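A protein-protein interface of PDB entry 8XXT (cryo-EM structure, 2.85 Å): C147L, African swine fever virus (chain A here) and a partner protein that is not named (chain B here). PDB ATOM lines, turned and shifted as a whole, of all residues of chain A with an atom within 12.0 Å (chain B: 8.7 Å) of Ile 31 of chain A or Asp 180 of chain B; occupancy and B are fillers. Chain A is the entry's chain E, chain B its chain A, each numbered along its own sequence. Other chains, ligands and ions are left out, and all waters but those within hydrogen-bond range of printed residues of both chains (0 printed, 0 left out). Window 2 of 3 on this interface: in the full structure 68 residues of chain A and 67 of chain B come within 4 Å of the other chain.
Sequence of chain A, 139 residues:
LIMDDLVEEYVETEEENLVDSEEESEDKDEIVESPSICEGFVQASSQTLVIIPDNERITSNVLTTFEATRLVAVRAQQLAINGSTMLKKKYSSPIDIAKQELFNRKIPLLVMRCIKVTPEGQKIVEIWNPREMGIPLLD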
ATOM      1  N   GLU A  30      -4.185  -1.092  34.578  1.00  0.00           N
ATOM      2  CA  GLU A  30      -4.154  -1.848  33.332  1.00  0.00           C
ATOM      3  C   GLU A  30      -4.520  -0.977  32.138  1.00  0.00           C
ATOM      4  O   GLU A  30      -5.695  -0.712  31.887  1.00  0.00           O
ATOM      5  CB  GLU A  30      -5.100  -3.048  33.405  1.00  0.00           C
ATOM      6  CG  GLU A  30      -5.181  -3.850  32.115  1.00  0.00           C
ATOM      7  CD  GLU A  30      -5.407  -5.326  32.358  1.00  0.00           C
ATOM      8  OE1 GLU A  30      -4.532  -5.970  32.973  1.00  0.00           O
ATOM      9  OE2 GLU A  30      -6.462  -5.844  31.938  1.00  0.00           O
ATOM     10  N   ILE A  31      -3.502  -0.531  31.403  1.00  0.00           N
ATOM     11  CA  ILE A  31      -3.756   0.209  30.174  1.00  0.00           C
ATOM     12  C   ILE A  31      -4.338  -0.717  29.109  1.00  0.00           C
ATOM     13  O   ILE A  31      -4.286  -1.949  29.208  1.00  0.00           O
ATOM     14  CB  ILE A  31      -2.480   0.918  29.684  1.00  0.00           C
ATOM     15  CG1 ILE A  31      -1.217   0.056  29.881  1.00  0.00           C
ATOM     16  CG2 ILE A  31      -2.326   2.264  30.374  1.00  0.00           C
ATOM     17  CD1 ILE A  31      -1.177  -1.280  29.157  1.00  0.00           C
ATOM     18  N   VAL A  32      -4.920  -0.108  28.079  1.00  0.00           N
ATOM     19  CA  VAL A  32      -5.594  -0.851  27.021  1.00  0.00           C
ATOM     20  C   VAL A  32      -5.366  -0.136  25.696  1.00  0.00           C
ATOM     21  O   VAL A  32      -5.248   1.093  25.650  1.00  0.00           O
ATOM     22  CB  VAL A  32      -7.101  -1.018  27.325  1.00  0.00           C
ATOM     23  CG1 VAL A  32      -7.753   0.328  27.592  1.00  0.00           C
ATOM     24  CG2 VAL A  32      -7.819  -1.774  26.205  1.00  0.00           C
ATOM     25  N   GLU A  33      -5.302  -0.914  24.623  1.00  0.00           N
ATOM     26  CA  GLU A  33      -5.120  -0.409  23.268  1.00  0.00           C
ATOM     27  C   GLU A  33      -5.932  -1.321  22.356  1.00  0.00           C
ATOM     28  O   GLU A  33      -6.867  -1.995  22.800  1.00  0.00           O
ATOM     29  CB  GLU A  33      -3.631  -0.338  22.896  1.00  0.00           C
ATOM     30  CG  GLU A  33      -3.173   1.047  22.459  1.00  0.00           C
ATOM     31  CD  GLU A  33      -1.716   1.077  22.037  1.00  0.00           C
ATOM     32  OE1 GLU A  33      -0.923   0.267  22.560  1.00  0.00           O
ATOM     33  OE2 GLU A  33      -1.361   1.914  21.181  1.00  0.00           O
ATOM     34  N   SER A  34      -5.613  -1.328  21.063  1.00  0.00           N
ATOM     35  CA  SER A  34      -6.383  -2.112  20.105  1.00  0.00           C
ATOM     36  C   SER A  34      -5.613  -3.351  19.668  1.00  0.00           C
ATOM     37  O   SER A  34      -4.745  -3.245  18.789  1.00  0.00           O
ATOM     38  CB  SER A  34      -6.737  -1.266  18.893  1.00  0.00           C
ATOM     39  OG  SER A  34      -7.567  -1.990  18.001  1.00  0.00           O
ATOM     40  N   PRO A  35      -5.883  -4.534  20.240  1.00  0.00           N
ATOM     41  CA  PRO A  35      -5.489  -5.775  19.568  1.00  0.00           C
ATOM     42  C   PRO A  35      -6.630  -6.300  18.716  1.00  0.00           C
ATOM     43  O   PRO A  35      -7.776  -5.870  18.880  1.00  0.00           O
ATOM     44  CB  PRO A  35      -5.169  -6.714  20.733  1.00  0.00           C
ATOM     45  CG  PRO A  35      -6.120  -6.281  21.798  1.00  0.00           C
ATOM     46  CD  PRO A  35      -6.368  -4.794  21.607  1.00  0.00           C
ATOM     47  N   CYS A  38      -7.475 -10.363  21.033  1.00  0.00           N
ATOM     48  CA  CYS A  38      -7.983 -10.380  22.401  1.00  0.00           C
ATOM     49  C   CYS A  38      -9.454  -9.986  22.445  1.00  0.00           C
ATOM     50  O   CYS A  38     -10.248 -10.610  23.156  1.00  0.00           O
ATOM     51  CB  CYS A  38      -7.152  -9.450  23.287  1.00  0.00           C
ATOM     52  SG  CYS A  38      -8.112  -8.505  24.497  1.00  0.00           S
ATOM     53  N   GLU A  39      -9.827  -8.956  21.694  1.00  0.00           N
ATOM     54  CA  GLU A  39     -11.218  -8.583  21.514  1.00  0.00           C
ATOM     55  C   GLU A  39     -11.733  -9.206  20.217  1.00  0.00           C
ATOM     56  O   GLU A  39     -11.072 -10.047  19.601  1.00  0.00           O
ATOM     57  CB  GLU A  39     -11.365  -7.063  21.531  1.00  0.00           C
ATOM     58  CG  GLU A  39     -10.657  -6.354  20.391  1.00  0.00           C
ATOM     59  CD  GLU A  39     -11.433  -5.157  19.875  1.00  0.00           C
ATOM     60  OE1 GLU A  39     -12.610  -4.998  20.260  1.00  0.00           O
ATOM     61  OE2 GLU A  39     -10.863  -4.370  19.090  1.00  0.00           O
ATOM     62  N   TRP B  94     -19.412  13.892  23.699  1.00  0.00           N
ATOM     63  CA  TRP B  94     -17.981  13.639  23.598  1.00  0.00           C
ATOM     64  C   TRP B  94     -17.183  14.921  23.427  1.00  0.00           C
ATOM     65  O   TRP B  94     -16.042  15.001  23.893  1.00  0.00           O
ATOM     66  CB  TRP B  94     -17.690  12.697  22.431  1.00  0.00           C
ATOM     67  CG  TRP B  94     -17.672  11.263  22.821  1.00  0.00           C
ATOM     68  CD1 TRP B  94     -18.525  10.292  22.400  1.00  0.00           C
ATOM     69  CD2 TRP B  94     -16.758  10.635  23.721  1.00  0.00           C
ATOM     70  NE1 TRP B  94     -18.198   9.092  22.980  1.00  0.00           N
ATOM     71  CE2 TRP B  94     -17.115   9.278  23.797  1.00  0.00           C
ATOM     72  CE3 TRP B  94     -15.672  11.087  24.470  1.00  0.00           C
ATOM     73  CZ2 TRP B  94     -16.425   8.369  24.590  1.00  0.00           C
ATOM     74  CZ3 TRP B  94     -14.987  10.184  25.255  1.00  0.00           C
ATOM     75  CH2 TRP B  94     -15.366   8.842  25.311  1.00  0.00           C
ATOM     76  N   GLY B 103      -6.696  16.190  22.942  1.00  0.00           N
ATOM     77  CA  GLY B 103      -7.411  14.936  23.019  1.00  0.00           C
ATOM     78  C   GLY B 103      -7.568  14.352  24.405  1.00  0.00           C
ATOM     79  O   GLY B 103      -8.466  13.529  24.613  1.00  0.00           O
ATOM     80  N   PRO B 105      -8.792  13.954  28.199  1.00  0.00           N
ATOM     81  CA  PRO B 105     -10.053  14.395  28.802  1.00  0.00           C
ATOM     82  C   PRO B 105      -9.840  15.567  29.744  1.00  0.00           C
ATOM     83  O   PRO B 105      -8.880  15.601  30.517  1.00  0.00           O
ATOM     84  CB  PRO B 105     -10.537  13.152  29.556  1.00  0.00           C
ATOM     85  CG  PRO B 105      -9.285  12.411  29.872  1.00  0.00           C
ATOM     86  CD  PRO B 105      -8.370  12.636  28.703  1.00  0.00           C
ATOM     87  N   LEU B 109     -11.012  11.575  35.189  1.00  0.00           N
ATOM     88  CA  LEU B 109     -11.400  10.181  35.002  1.00  0.00           C
ATOM     89  C   LEU B 109     -11.411   9.420  36.321  1.00  0.00           C
ATOM     90  O   LEU B 109     -12.117   8.415  36.451  1.00  0.00           O
ATOM     91  CB  LEU B 109     -10.459   9.500  34.011  1.00  0.00           C
ATOM     92  CG  LEU B 109     -10.450  10.030  32.578  1.00  0.00           C
ATOM     93  CD1 LEU B 109      -9.582   9.148  31.699  1.00  0.00           C
ATOM     94  CD2 LEU B 109     -11.861  10.120  32.026  1.00  0.00           C
ATOM     95  N   GLU B 113     -15.031   6.857  38.193  1.00  0.00           N
ATOM     96  CA  GLU B 113     -14.874   5.407  38.197  1.00  0.00           C
ATOM     97  C   GLU B 113     -16.008   4.724  38.952  1.00  0.00           C
ATOM     98  O   GLU B 113     -16.529   3.694  38.509  1.00  0.00           O
ATOM     99  CB  GLU B 113     -13.524   5.036  38.806  1.00  0.00           C
ATOM    100  CG  GLU B 113     -12.382   5.016  37.812  1.00  0.00           C
ATOM    101  CD  GLU B 113     -12.220   3.665  37.153  1.00  0.00           C
ATOM    102  OE1 GLU B 113     -12.917   2.715  37.572  1.00  0.00           O
ATOM    103  OE2 GLU B 113     -11.397   3.549  36.220  1.00  0.00           O
ATOM    104  N   ARG B 117     -20.521   1.914  34.169  1.00  0.00           N
ATOM    105  CA  ARG B 117     -19.932   2.259  32.878  1.00  0.00           C
ATOM    106  C   ARG B 117     -20.893   2.954  31.917  1.00  0.00           C
ATOM    107  O   ARG B 117     -20.471   3.938  31.283  1.00  0.00           O
ATOM    108  CB  ARG B 117     -19.338   1.002  32.233  1.00  0.00           C
ATOM    109  CG  ARG B 117     -18.487   0.171  33.176  1.00  0.00           C
ATOM    110  CD  ARG B 117     -17.787  -0.950  32.436  1.00  0.00           C
ATOM    111  NE  ARG B 117     -16.729  -0.444  31.572  1.00  0.00           N
ATOM    112  CZ  ARG B 117     -16.815  -0.361  30.252  1.00  0.00           C
ATOM    113  NH1 ARG B 117     -17.903  -0.747  29.605  1.00  0.00           N
ATOM    114  NH2 ARG B 117     -15.787   0.123  29.563  1.00  0.00           N
ATOM    115  N   ARG B 120     -21.212   6.798  32.801  1.00  0.00           N
ATOM    116  CA  ARG B 120     -20.022   7.603  33.074  1.00  0.00           C
ATOM    117  C   ARG B 120     -19.914   8.780  32.116  1.00  0.00           C
ATOM    118  O   ARG B 120     -19.668   9.916  32.536  1.00  0.00           O
ATOM    119  CB  ARG B 120     -18.767   6.739  32.982  1.00  0.00           C
ATOM    120  CG  ARG B 120     -18.476   5.901  34.203  1.00  0.00           C
ATOM    121  CD  ARG B 120     -17.163   5.170  34.028  1.00  0.00           C
ATOM    122  NE  ARG B 120     -17.050   4.016  34.909  1.00  0.00           N
ATOM    123  CZ  ARG B 120     -16.140   3.062  34.773  1.00  0.00           C
ATOM    124  NH1 ARG B 120     -15.246   3.094  33.801  1.00  0.00           N
ATOM    125  NH2 ARG B 120     -16.127   2.050  35.635  1.00  0.00           N
ATOM    126  N   VAL B 177      -8.382  11.324  20.382  1.00  0.00           N
ATOM    127  CA  VAL B 177      -8.765  10.642  21.614  1.00  0.00           C
ATOM    128  C   VAL B 177      -8.165   9.244  21.642  1.00  0.00           C
ATOM    129  O   VAL B 177      -8.171   8.524  20.637  1.00  0.00           O
ATOM    130  CB  VAL B 177     -10.295  10.591  21.747  1.00  0.00           C
ATOM    131  CG1 VAL B 177     -10.690  10.005  23.089  1.00  0.00           C
ATOM    132  CG2 VAL B 177     -10.876  11.975  21.583  1.00  0.00           C
ATOM    133  N   THR B 178      -7.648   8.855  22.802  1.00  0.00           N
ATOM    134  CA  THR B 178      -7.066   7.538  22.994  1.00  0.00           C
ATOM    135  C   THR B 178      -8.116   6.553  23.498  1.00  0.00           C
ATOM    136  O   THR B 178      -9.194   6.936  23.956  1.00  0.00           O
ATOM    137  CB  THR B 178      -5.899   7.599  23.978  1.00  0.00           C
ATOM    138  OG1 THR B 178      -5.553   6.273  24.394  1.00  0.00           O
ATOM    139  CG2 THR B 178      -6.279   8.421  25.194  1.00  0.00           C
ATOM    140  N   TYR B 179      -7.777   5.265  23.413  1.00  0.00           N
ATOM    141  CA  TYR B 179      -8.698   4.226  23.860  1.00  0.00           C
ATOM    142  C   TYR B 179      -8.864   4.227  25.373  1.00  0.00           C
ATOM    143  O   TYR B 179      -9.908   3.800  25.877  1.00  0.00           O
ATOM    144  CB  TYR B 179      -8.215   2.857  23.388  1.00  0.00           C
ATOM    145  CG  TYR B 179      -8.563   2.547  21.954  1.00  0.00           C
ATOM    146  CD1 TYR B 179      -9.880   2.361  21.565  1.00  0.00           C
ATOM    147  CD2 TYR B 179      -7.575   2.442  20.989  1.00  0.00           C
ATOM    148  CE1 TYR B 179     -10.201   2.079  20.256  1.00  0.00           C
ATOM    149  CE2 TYR B 179      -7.887   2.158  19.678  1.00  0.00           C
ATOM    150  CZ  TYR B 179      -9.200   1.977  19.317  1.00  0.00           C
ATOM    151  OH  TYR B 179      -9.510   1.694  18.008  1.00  0.00           O
ATOM    152  N   ASP B 180      -7.848   4.685  26.108  1.00  0.00           N
ATOM    153  CA  ASP B 180      -7.949   4.716  27.563  1.00  0.00           C
ATOM    154  C   ASP B 180      -9.075   5.631  28.017  1.00  0.00           C
ATOM    155  O   ASP B 180      -9.814   5.301  28.949  1.00  0.00           O
ATOM    156  CB  ASP B 180      -6.624   5.163  28.175  1.00  0.00           C
ATOM    157  CG  ASP B 180      -5.899   4.037  28.870  1.00  0.00           C
ATOM    158  OD1 ASP B 180      -6.202   2.866  28.571  1.00  0.00           O
ATOM    159  OD2 ASP B 180      -5.031   4.321  29.720  1.00  0.00           O
ATOM    160  N   THR B 181      -9.215   6.790  27.375  1.00  0.00           N
ATOM    161  CA  THR B 181     -10.309   7.693  27.715  1.00  0.00           C
ATOM    162  C   THR B 181     -11.658   7.053  27.421  1.00  0.00           C
ATOM    163  O   THR B 181     -12.604   7.196  28.203  1.00  0.00           O
ATOM    164  CB  THR B 181     -10.159   9.005  26.948  1.00  0.00           C
ATOM    165  OG1 THR B 181      -8.834   9.517  27.130  1.00  0.00           O
ATOM    166  CG2 THR B 181     -11.160  10.028  27.447  1.00  0.00           C
ATOM    167  N   VAL B 182     -11.764   6.343  26.296  1.00  0.00           N
ATOM    168  CA  VAL B 182     -13.024   5.699  25.932  1.00  0.00           C
ATOM    169  C   VAL B 182     -13.395   4.635  26.955  1.00  0.00           C
ATOM    170  O   VAL B 182     -14.544   4.552  27.403  1.00  0.00           O
ATOM    171  CB  VAL B 182     -12.928   5.097  24.521  1.00  0.00           C
ATOM    172  CG1 VAL B 182     -14.294   4.662  24.043  1.00  0.00           C
ATOM    173  CG2 VAL B 182     -12.316   6.093  23.570  1.00  0.00           C
ATOM    174  N   VAL B 183     -12.431   3.797  27.332  1.00  0.00           N
ATOM    175  CA  VAL B 183     -12.720   2.715  28.266  1.00  0.00           C
ATOM    176  C   VAL B 183     -13.032   3.271  29.649  1.00  0.00           C
ATOM    177  O   VAL B 183     -14.009   2.868  30.290  1.00  0.00           O
ATOM    178  CB  VAL B 183     -11.552   1.715  28.308  1.00  0.00           C
ATOM    179  CG1 VAL B 183     -11.857   0.592  29.275  1.00  0.00           C
ATOM    180  CG2 VAL B 183     -11.298   1.155  26.927  1.00  0.00           C
ATOM    181  N   LYS B 184     -12.218   4.215  30.126  1.00  0.00           N
ATOM    182  CA  LYS B 184     -12.408   4.749  31.467  1.00  0.00           C
ATOM    183  C   LYS B 184     -13.657   5.606  31.579  1.00  0.00           C
ATOM    184  O   LYS B 184     -14.090   5.905  32.696  1.00  0.00           O
ATOM    185  CB  LYS B 184     -11.178   5.547  31.893  1.00  0.00           C
ATOM    186  CG  LYS B 184      -9.964   4.680  32.178  1.00  0.00           C
ATOM    187  CD  LYS B 184      -8.707   5.509  32.339  1.00  0.00           C
ATOM    188  CE  LYS B 184      -7.467   4.633  32.287  1.00  0.00           C
ATOM    189  NZ  LYS B 184      -7.431   3.653  33.407  1.00  0.00           N
ATOM    190  N   LEU B 185     -14.242   6.009  30.456  1.00  0.00           N
ATOM    191  CA  LEU B 185     -15.540   6.664  30.452  1.00  0.00           C
ATOM    192  C   LEU B 185     -16.676   5.690  30.178  1.00  0.00           C
ATOM    193  O   LEU B 185     -17.810   6.122  29.953  1.00  0.00           O
ATOM    194  CB  LEU B 185     -15.559   7.798  29.429  1.00  0.00           C
ATOM    195  CG  LEU B 185     -14.870   9.078  29.894  1.00  0.00           C
ATOM    196  CD1 LEU B 185     -14.608   9.993  28.721  1.00  0.00           C
ATOM    197  CD2 LEU B 185     -15.709   9.781  30.943  1.00  0.00           C
ATOM    198  N   GLY B 186     -16.391   4.390  30.169  1.00  0.00           N
ATOM    199  CA  GLY B 186     -17.406   3.373  30.076  1.00  0.00           C
ATOM    200  C   GLY B 186     -17.787   2.966  28.671  1.00  0.00           C
ATOM    201  O   GLY B 186     -18.331   1.873  28.487  1.00  0.00           O
ATOM    202  N   ARG B 187     -17.515   3.803  27.678  1.00  0.00           N
ATOM    203  CA  ARG B 187     -17.869   3.459  26.311  1.00  0.00           C
ATOM    204  C   ARG B 187     -17.055   2.266  25.835  1.00  0.00           C
ATOM    205  O   ARG B 187     -15.884   2.103  26.182  1.00  0.00           O
ATOM    206  CB  ARG B 187     -17.647   4.649  25.384  1.00  0.00           C
ATOM    207  CG  ARG B 187     -18.744   5.682  25.452  1.00  0.00           C
ATOM    208  CD  ARG B 187     -20.035   5.142  24.879  1.00  0.00           C
ATOM    209  NE  ARG B 187     -21.127   6.095  25.023  1.00  0.00           N
ATOM    210  CZ  ARG B 187     -22.140   5.947  25.864  1.00  0.00           C
ATOM    211  NH1 ARG B 187     -22.236   4.889  26.650  1.00  0.00           N
ATOM    212  NH2 ARG B 187     -23.081   6.885  25.918  1.00  0.00           N
ATOM    213  N   LYS B 189     -14.916  -0.187  23.400  1.00  0.00           N
ATOM    214  CA  LYS B 189     -13.835   0.086  22.463  1.00  0.00           C
ATOM    215  C   LYS B 189     -14.339   0.142  21.028  1.00  0.00           C
ATOM    216  O   LYS B 189     -13.765   0.853  20.196  1.00  0.00           O
ATOM    217  CB  LYS B 189     -12.750  -0.973  22.604  1.00  0.00           C
ATOM    218  CG  LYS B 189     -11.446  -0.446  23.147  1.00  0.00           C
ATOM    219  CD  LYS B 189     -10.495  -1.590  23.389  1.00  0.00           C
ATOM    220  CE  LYS B 189     -10.139  -2.260  22.083  1.00  0.00           C
ATOM    221  NZ  LYS B 189      -8.821  -2.915  22.166  1.00  0.00           N
ATOM    222  N   HIS B 192     -15.716   3.843  19.858  1.00  0.00           N
ATOM    223  CA  HIS B 192     -14.756   4.932  19.924  1.00  0.00           C
ATOM    224  C   HIS B 192     -15.338   6.176  19.257  1.00  0.00           C
ATOM    225  O   HIS B 192     -16.034   6.066  18.242  1.00  0.00           O
ATOM    226  CB  HIS B 192     -13.451   4.525  19.238  1.00  0.00           C
ATOM    227  CG  HIS B 192     -12.302   5.437  19.533  1.00  0.00           C
ATOM    228  ND1 HIS B 192     -12.137   6.653  18.905  1.00  0.00           N
ATOM    229  CD2 HIS B 192     -11.261   5.312  20.388  1.00  0.00           C
ATOM    230  CE1 HIS B 192     -11.045   7.237  19.362  1.00  0.00           C
ATOM    231  NE2 HIS B 192     -10.494   6.443  20.263  1.00  0.00           N
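The guanidinium group (NH2) of Arg 117 of chain B sits at hydrogen-bond distance from the backbone carbonyl oxygen (O) of Val 183 of chain B (3.4 Å). The side-chain hydroxyl (OG1) of Thr 178 of chain B lies close to the backbone NH (N) of Asp 180 of chain B, 3.3 Å away.
CG2 of Ile 31 of chain A touches OD2 of Asp 180 of chain B, at 3.5 Å. Val 183 of chain B touches Val 32 of chain A (CG2 to CG1, 3.7 Å). CG2 of Val 32 of chain A touches CD of Lys 189 of chain B, at 3.9 Å. CE2 of Tyr 179 of chain B touches CB of Ser 34 of chain A, at 3.7 Å. CA of Ser 34 of chain A touches NZ of Lys 189 of chain B, 3.3 Å away. Pro 35 of chain A touches Lys 189 of chain B (CD to NZ, 3.1 Å).
OD1 of Asp 180 of chain B sits close to N of Val 32 of chain A, at 3.3 Å. The side-chain carboxylate (OE2) of Glu 39 of chain A lies within salt-bridge range of the side-chain amino group (NZ) of Lys 189 of chain B, 3.97 Å away. O of Glu 33 of chain A lies close to NZ of Lys 189 of chain B, at 2.3 Å.
Of chain B, only Asp 180 (3.5 Å) comes within 4 Å of Ile 31 of chain A. Printed residues of chain A within 4 Å of Asp 180 of chain B: Ile 31 and Val 32. No residue of chain A comes within 4 Å of Thr 178 of chain B. No residue of chain A comes within 4 Å of Thr 181 of chain B. Val 183 of chain B touches one residue of chain A. No residue of chain A comes within 4 Å of Lys 184 of chain B. Of the printed residues of chain B, Ser 34 of chain A touches Tyr 179 and Lys 189. Of the printed residues of chain B, Glu 33 of chain A touches Lys 189 (2.3 Å). Of the printed residues of chain A, Tyr 179 of chain B touches Ser 34 (3.7 Å). Printed residues of chain B within 4 Å of Pro 35 of chain A: Lys 189. Printed residues of chain A within 4 Å of Lys 189 of chain B: Val 32 (3.9 Å), Glu 33 (2.3 Å), Ser 34 (3.3 Å), Pro 35 (3.1 Å) and Glu 39 (3.7 Å). Arg 187 of chain B touches none of the printed residues of chain A. The nearest residue of chain A that does not touch Asp 180 of chain B is Glu 30 of chain A (4.9 Å).
Hydrophobic or aromatic side chains of chain A that line the printed part of chain B: Ile 31, Val 32 and Pro 35. Along chain A the printed residues that touch a printed residue of chain B span positions 31 to 39. Hydrophobic or aromatic side chains of chain B within 4 Å of the printed part of chain A: Tyr 179 and Val 183. Along chain B the printed residues that touch a printed residue of chain A span positions 179 to 189. Among the printed residues, Asp or Glu carboxylates within 4 Å of a Lys or Arg side-chain nitrogen of the other chain: Glu 39 of chain A with Lys 189 of chain B.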
